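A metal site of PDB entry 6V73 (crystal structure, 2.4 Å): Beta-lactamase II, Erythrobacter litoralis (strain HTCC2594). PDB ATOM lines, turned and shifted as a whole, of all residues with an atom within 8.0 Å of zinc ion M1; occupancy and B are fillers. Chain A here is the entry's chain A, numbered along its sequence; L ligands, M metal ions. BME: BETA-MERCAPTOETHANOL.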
ATOM      1  N   TRP A  69       9.575 -13.150 -17.099  1.00  0.00           N
ATOM      2  CA  TRP A  69       9.138 -14.552 -17.124  1.00  0.00           C
ATOM      3  C   TRP A  69       8.020 -14.827 -16.128  1.00  0.00           C
ATOM      4  O   TRP A  69       7.165 -15.682 -16.385  1.00  0.00           O
ATOM      5  CB  TRP A  69      10.306 -15.489 -16.844  1.00  0.00           C
ATOM      6  CG  TRP A  69      11.383 -15.582 -17.906  1.00  0.00           C
ATOM      7  CD1 TRP A  69      12.527 -14.844 -17.982  1.00  0.00           C
ATOM      8  CD2 TRP A  69      11.428 -16.518 -18.996  1.00  0.00           C
ATOM      9  NE1 TRP A  69      13.274 -15.234 -19.078  1.00  0.00           N
ATOM     10  CE2 TRP A  69      12.629 -16.261 -19.713  1.00  0.00           C
ATOM     11  CE3 TRP A  69      10.576 -17.532 -19.444  1.00  0.00           C
ATOM     12  CZ2 TRP A  69      12.988 -16.985 -20.871  1.00  0.00           C
ATOM     13  CZ3 TRP A  69      10.943 -18.255 -20.607  1.00  0.00           C
ATOM     14  CH2 TRP A  69      12.141 -17.986 -21.290  1.00  0.00           C
ATOM     15  N   THR A  95       4.315  -9.424 -27.155  1.00  0.00           N
ATOM     16  CA  THR A  95       4.630  -9.702 -28.549  1.00  0.00           C
ATOM     17  C   THR A  95       4.224 -11.099 -29.016  1.00  0.00           C
ATOM     18  O   THR A  95       4.260 -11.342 -30.232  1.00  0.00           O
ATOM     19  CB  THR A  95       6.120  -9.470 -28.828  1.00  0.00           C
ATOM     20  OG1 THR A  95       6.921  -9.995 -27.768  1.00  0.00           O
ATOM     21  CG2 THR A  95       6.373  -7.979 -28.903  1.00  0.00           C
ATOM     22  N   HIS A  96       3.841 -12.018 -28.107  1.00  0.00           N
ATOM     23  CA  HIS A  96       3.119 -13.248 -28.428  1.00  0.00           C
ATOM     24  C   HIS A  96       2.882 -14.091 -27.172  1.00  0.00           C
ATOM     25  O   HIS A  96       3.361 -13.745 -26.086  1.00  0.00           O
ATOM     26  CB  HIS A  96       3.833 -14.110 -29.485  1.00  0.00           C
ATOM     27  CG  HIS A  96       5.191 -14.572 -29.067  1.00  0.00           C
ATOM     28  ND1 HIS A  96       6.303 -13.758 -29.129  1.00  0.00           N
ATOM     29  CD2 HIS A  96       5.629 -15.756 -28.583  1.00  0.00           C
ATOM     30  CE1 HIS A  96       7.357 -14.423 -28.700  1.00  0.00           C
ATOM     31  NE2 HIS A  96       6.976 -15.647 -28.369  1.00  0.00           N
ATOM     32  N   ALA A  97       2.167 -15.202 -27.321  1.00  0.00           N
ATOM     33  CA  ALA A  97       1.682 -15.984 -26.177  1.00  0.00           C
ATOM     34  C   ALA A  97       2.698 -17.056 -25.782  1.00  0.00           C
ATOM     35  O   ALA A  97       2.453 -18.257 -25.879  1.00  0.00           O
ATOM     36  CB  ALA A  97       0.324 -16.602 -26.490  1.00  0.00           C
ATOM     37  N   HIS A  98       3.852 -16.603 -25.313  1.00  0.00           N
ATOM     38  CA  HIS A  98       4.812 -17.494 -24.674  1.00  0.00           C
ATOM     39  C   HIS A  98       5.196 -16.893 -23.326  1.00  0.00           C
ATOM     40  O   HIS A  98       5.031 -15.694 -23.092  1.00  0.00           O
ATOM     41  CB  HIS A  98       6.100 -17.723 -25.521  1.00  0.00           C
ATOM     42  CG  HIS A  98       5.952 -18.768 -26.584  1.00  0.00           C
ATOM     43  ND1 HIS A  98       6.868 -18.900 -27.607  1.00  0.00           N
ATOM     44  CD2 HIS A  98       5.010 -19.725 -26.786  1.00  0.00           C
ATOM     45  CE1 HIS A  98       6.486 -19.893 -28.404  1.00  0.00           C
ATOM     46  NE2 HIS A  98       5.359 -20.398 -27.925  1.00  0.00           N
ATOM     47  N   GLN A  99       5.745 -17.738 -22.465  1.00  0.00           N
ATOM     48  CA  GLN A  99       5.930 -17.341 -21.074  1.00  0.00           C
ATOM     49  C   GLN A  99       6.950 -16.232 -20.911  1.00  0.00           C
ATOM     50  O   GLN A  99       6.806 -15.399 -19.999  1.00  0.00           O
ATOM     51  CB  GLN A  99       6.316 -18.540 -20.218  1.00  0.00           C
ATOM     52  CG  GLN A  99       6.169 -18.223 -18.745  1.00  0.00           C
ATOM     53  CD  GLN A  99       6.842 -19.244 -17.883  1.00  0.00           C
ATOM     54  OE1 GLN A  99       6.921 -20.423 -18.236  1.00  0.00           O
ATOM     55  NE2 GLN A  99       7.356 -18.792 -16.749  1.00  0.00           N
ATOM     56  N   ASP A 100       7.992 -16.182 -21.744  1.00  0.00           N
ATOM     57  CA  ASP A 100       8.945 -15.080 -21.573  1.00  0.00           C
ATOM     58  C   ASP A 100       8.336 -13.723 -21.931  1.00  0.00           C
ATOM     59  O   ASP A 100       8.852 -12.703 -21.489  1.00  0.00           O
ATOM     60  CB  ASP A 100      10.216 -15.321 -22.394  1.00  0.00           C
ATOM     61  CG  ASP A 100       9.938 -15.744 -23.804  1.00  0.00           C
ATOM     62  OD1 ASP A 100      10.795 -15.485 -24.668  1.00  0.00           O
ATOM     63  OD2 ASP A 100       8.863 -16.346 -24.056  1.00  0.00           O
ATOM     64  N   LYS A 101       7.252 -13.696 -22.728  1.00  0.00           N
ATOM     65  CA  LYS A 101       6.637 -12.426 -23.121  1.00  0.00           C
ATOM     66  C   LYS A 101       5.350 -12.111 -22.356  1.00  0.00           C
ATOM     67  O   LYS A 101       5.027 -10.919 -22.214  1.00  0.00           O
ATOM     68  CB  LYS A 101       6.363 -12.401 -24.642  1.00  0.00           C
ATOM     69  CG  LYS A 101       7.625 -12.588 -25.531  1.00  0.00           C
ATOM     70  CD  LYS A 101       8.863 -12.031 -24.816  1.00  0.00           C
ATOM     71  CE  LYS A 101       9.739 -11.176 -25.668  1.00  0.00           C
ATOM     72  NZ  LYS A 101      10.982 -10.826 -24.954  1.00  0.00           N
ATOM     73  N   HIS A 165       8.186 -16.902 -35.748  1.00  0.00           N
ATOM     74  CA  HIS A 165       8.478 -17.618 -34.504  1.00  0.00           C
ATOM     75  C   HIS A 165       7.211 -18.222 -33.901  1.00  0.00           C
ATOM     76  O   HIS A 165       7.243 -19.356 -33.405  1.00  0.00           O
ATOM     77  CB  HIS A 165       9.163 -16.676 -33.511  1.00  0.00           C
ATOM     78  CG  HIS A 165       9.216 -17.215 -32.113  1.00  0.00           C
ATOM     79  ND1 HIS A 165      10.065 -18.238 -31.733  1.00  0.00           N
ATOM     80  CD2 HIS A 165       8.515 -16.874 -30.998  1.00  0.00           C
ATOM     81  CE1 HIS A 165       9.892 -18.492 -30.455  1.00  0.00           C
ATOM     82  NE2 HIS A 165       8.955 -17.684 -29.981  1.00  0.00           N
ATOM     83  N   THR A 166       6.101 -17.477 -33.918  1.00  0.00           N
ATOM     84  CA  THR A 166       4.768 -18.015 -33.699  1.00  0.00           C
ATOM     85  C   THR A 166       3.818 -17.357 -34.685  1.00  0.00           C
ATOM     86  O   THR A 166       4.183 -16.416 -35.396  1.00  0.00           O
ATOM     87  CB  THR A 166       4.257 -17.786 -32.266  1.00  0.00           C
ATOM     88  OG1 THR A 166       4.118 -16.386 -32.061  1.00  0.00           O
ATOM     89  CG2 THR A 166       5.189 -18.350 -31.207  1.00  0.00           C
ATOM     90  N   ASP A 168       1.251 -15.623 -33.909  1.00  0.00           N
ATOM     91  CA  ASP A 168       0.760 -14.380 -33.349  1.00  0.00           C
ATOM     92  C   ASP A 168       1.844 -13.339 -33.076  1.00  0.00           C
ATOM     93  O   ASP A 168       1.511 -12.265 -32.551  1.00  0.00           O
ATOM     94  CB  ASP A 168      -0.018 -14.656 -32.049  1.00  0.00           C
ATOM     95  CG  ASP A 168       0.837 -15.386 -31.009  1.00  0.00           C
ATOM     96  OD1 ASP A 168       1.716 -16.183 -31.402  1.00  0.00           O
ATOM     97  OD2 ASP A 168       0.624 -15.180 -29.794  1.00  0.00           O
ATOM     98  N   ASN A 169       3.112 -13.605 -33.420  1.00  0.00           N
ATOM     99  CA  ASN A 169       4.164 -12.675 -32.992  1.00  0.00           C
ATOM    100  C   ASN A 169       3.989 -11.311 -33.647  1.00  0.00           C
ATOM    101  O   ASN A 169       3.719 -11.196 -34.844  1.00  0.00           O
ATOM    102  CB  ASN A 169       5.586 -13.168 -33.305  1.00  0.00           C
ATOM    103  CG  ASN A 169       5.801 -13.580 -34.761  1.00  0.00           C
ATOM    104  OD1 ASN A 169       5.964 -14.753 -35.060  1.00  0.00           O
ATOM    105  ND2 ASN A 169       5.733 -12.623 -35.673  1.00  0.00           N
ATOM    106  N   GLY A 183      11.188  -8.898 -31.248  1.00  0.00           N
ATOM    107  CA  GLY A 183      10.745  -9.972 -30.385  1.00  0.00           C
ATOM    108  C   GLY A 183      11.607 -11.210 -30.540  1.00  0.00           C
ATOM    109  O   GLY A 183      12.836 -11.129 -30.690  1.00  0.00           O
ATOM    110  N   CYS A 184      10.956 -12.360 -30.479  1.00  0.00           N
ATOM    111  CA  CYS A 184      11.591 -13.658 -30.645  1.00  0.00           C
ATOM    112  C   CYS A 184      11.712 -14.084 -32.099  1.00  0.00           C
ATOM    113  O   CYS A 184      12.383 -15.082 -32.373  1.00  0.00           O
ATOM    114  CB  CYS A 184      10.837 -14.727 -29.878  1.00  0.00           C
ATOM    115  SG  CYS A 184      10.646 -14.388 -28.118  1.00  0.00           S
ATOM    116  N   MET A 185      11.071 -13.351 -33.021  1.00  0.00           N
ATOM    117  CA  MET A 185      11.222 -13.672 -34.435  1.00  0.00           C
ATOM    118  C   MET A 185      12.647 -13.441 -34.901  1.00  0.00           C
ATOM    119  O   MET A 185      13.185 -14.214 -35.701  1.00  0.00           O
ATOM    120  CB  MET A 185      10.258 -12.839 -35.262  1.00  0.00           C
ATOM    121  CG  MET A 185      10.526 -12.908 -36.750  1.00  0.00           C
ATOM    122  SD  MET A 185       9.309 -12.040 -37.741  1.00  0.00           S
ATOM    123  CE  MET A 185       9.729 -10.337 -37.394  1.00  0.00           C
ATOM    124  N   LYS A 187      16.663 -13.199 -34.487  1.00  0.00           N
ATOM    125  CA  LYS A 187      17.748 -13.777 -33.713  1.00  0.00           C
ATOM    126  C   LYS A 187      19.054 -13.094 -34.107  1.00  0.00           C
ATOM    127  O   LYS A 187      19.102 -12.307 -35.062  1.00  0.00           O
ATOM    128  CB  LYS A 187      17.810 -15.289 -33.903  1.00  0.00           C
ATOM    129  CG  LYS A 187      17.260 -16.084 -32.714  1.00  0.00           C
ATOM    130  CD  LYS A 187      15.740 -16.170 -32.706  1.00  0.00           C
ATOM    131  CE  LYS A 187      15.276 -16.713 -31.367  1.00  0.00           C
ATOM    132  NZ  LYS A 187      13.979 -17.422 -31.455  1.00  0.00           N
ATOM    133  N   ASN A 196      13.556 -21.578 -30.458  1.00  0.00           N
ATOM    134  CA  ASN A 196      12.462 -22.506 -30.186  1.00  0.00           C
ATOM    135  C   ASN A 196      11.407 -22.391 -31.276  1.00  0.00           C
ATOM    136  O   ASN A 196      10.625 -21.437 -31.307  1.00  0.00           O
ATOM    137  CB  ASN A 196      11.870 -22.240 -28.807  1.00  0.00           C
ATOM    138  CG  ASN A 196      10.540 -22.935 -28.613  1.00  0.00           C
ATOM    139  OD1 ASN A 196      10.323 -24.056 -29.097  1.00  0.00           O
ATOM    140  ND2 ASN A 196       9.633 -22.276 -27.905  1.00  0.00           N
ATOM    141  N   LEU A 197      11.344 -23.409 -32.134  1.00  0.00           N
ATOM    142  CA  LEU A 197      10.440 -23.446 -33.281  1.00  0.00           C
ATOM    143  C   LEU A 197       9.190 -24.302 -33.037  1.00  0.00           C
ATOM    144  O   LEU A 197       8.450 -24.570 -33.978  1.00  0.00           O
ATOM    145  CB  LEU A 197      11.184 -23.982 -34.520  1.00  0.00           C
ATOM    146  CG  LEU A 197      12.344 -23.154 -35.086  1.00  0.00           C
ATOM    147  CD1 LEU A 197      12.916 -23.770 -36.367  1.00  0.00           C
ATOM    148  CD2 LEU A 197      11.937 -21.715 -35.337  1.00  0.00           C
ATOM    149  N   ASP A 199       6.262 -23.807 -31.927  1.00  0.00           N
ATOM    150  CA  ASP A 199       5.022 -23.227 -32.423  1.00  0.00           C
ATOM    151  C   ASP A 199       5.243 -22.366 -33.662  1.00  0.00           C
ATOM    152  O   ASP A 199       4.374 -21.563 -34.012  1.00  0.00           O
ATOM    153  CB  ASP A 199       4.332 -22.388 -31.340  1.00  0.00           C
ATOM    154  CG  ASP A 199       4.132 -23.156 -30.040  1.00  0.00           C
ATOM    155  OD1 ASP A 199       3.636 -24.295 -30.091  1.00  0.00           O
ATOM    156  OD2 ASP A 199       4.484 -22.606 -28.973  1.00  0.00           O
ATOM    157  N   SER A 225      14.513 -10.576 -28.333  1.00  0.00           N
ATOM    158  CA  SER A 225      14.166 -11.144 -27.027  1.00  0.00           C
ATOM    159  C   SER A 225      15.348 -11.817 -26.338  1.00  0.00           C
ATOM    160  O   SER A 225      15.423 -11.803 -25.100  1.00  0.00           O
ATOM    161  CB  SER A 225      13.040 -12.154 -27.172  1.00  0.00           C
ATOM    162  OG  SER A 225      11.865 -11.537 -27.670  1.00  0.00           O
ATOM    163  N   HIS A 226      16.261 -12.446 -27.082  1.00  0.00           N
ATOM    164  CA  HIS A 226      17.158 -13.393 -26.426  1.00  0.00           C
ATOM    165  C   HIS A 226      18.638 -13.108 -26.651  1.00  0.00           C
ATOM    166  O   HIS A 226      19.471 -13.950 -26.293  1.00  0.00           O
ATOM    167  CB  HIS A 226      16.815 -14.833 -26.849  1.00  0.00           C
ATOM    168  CG  HIS A 226      15.450 -15.258 -26.409  1.00  0.00           C
ATOM    169  ND1 HIS A 226      15.094 -15.370 -25.087  1.00  0.00           N
ATOM    170  CD2 HIS A 226      14.335 -15.564 -27.118  1.00  0.00           C
ATOM    171  CE1 HIS A 226      13.824 -15.747 -24.996  1.00  0.00           C
ATOM    172  NE2 HIS A 226      13.343 -15.876 -26.217  1.00  0.00           N
HETATM  173  C1  BME L   1      10.133 -20.018 -25.658  1.00  0.00           C
HETATM  174  C2  BME L   1      10.448 -19.152 -26.884  1.00  0.00           C
HETATM  175  O1  BME L   1      11.325 -20.292 -24.941  1.00  0.00           O
HETATM  176  S2  BME L   1       9.801 -17.448 -26.665  1.00  0.00           S
HETATM  177 ZN    ZN M   1       8.228 -17.356 -28.039  1.00  0.00          ZN
HETATM  178 ZN    ZN M   2      11.395 -16.205 -26.953  1.00  0.00          ZN
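N of His 165 is in hydrogen-bond range of OD1 of Asn 169 (3.2 Å). The backbone carbonyl oxygen (O) of Asn 196 sits close to a ring nitrogen (ND1) of His 165 (3.3 Å). OG of Ser 225 sits at hydrogen-bond distance from N of Cys 184 (3.1 Å). NE2 of His 98 lies within hydrogen-bond range of OD2 of Asp 199 (2.6 Å). NZ of Lys 187 lies within hydrogen-bond range of O of Cys 184, 3.0 Å away.
Cys 184 touches zinc ion M1 (SG to ZN, 3.8 Å). The nearest printed residue that does not touch zinc ion M1 is Asp 100 (4.2 Å).
A sulfur (S2) of the ligand is bound to zinc ion M1 (2.1 Å). Zinc ion M1 is bound by NE2 of His 165 (2.1 Å). Zinc ion M1 is bound by ND1 of His 98. Zinc ion M1 is bound by NE2 of His 96, 2.1 Å away. Zinc ion M1 has four donor atoms within binding distance.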
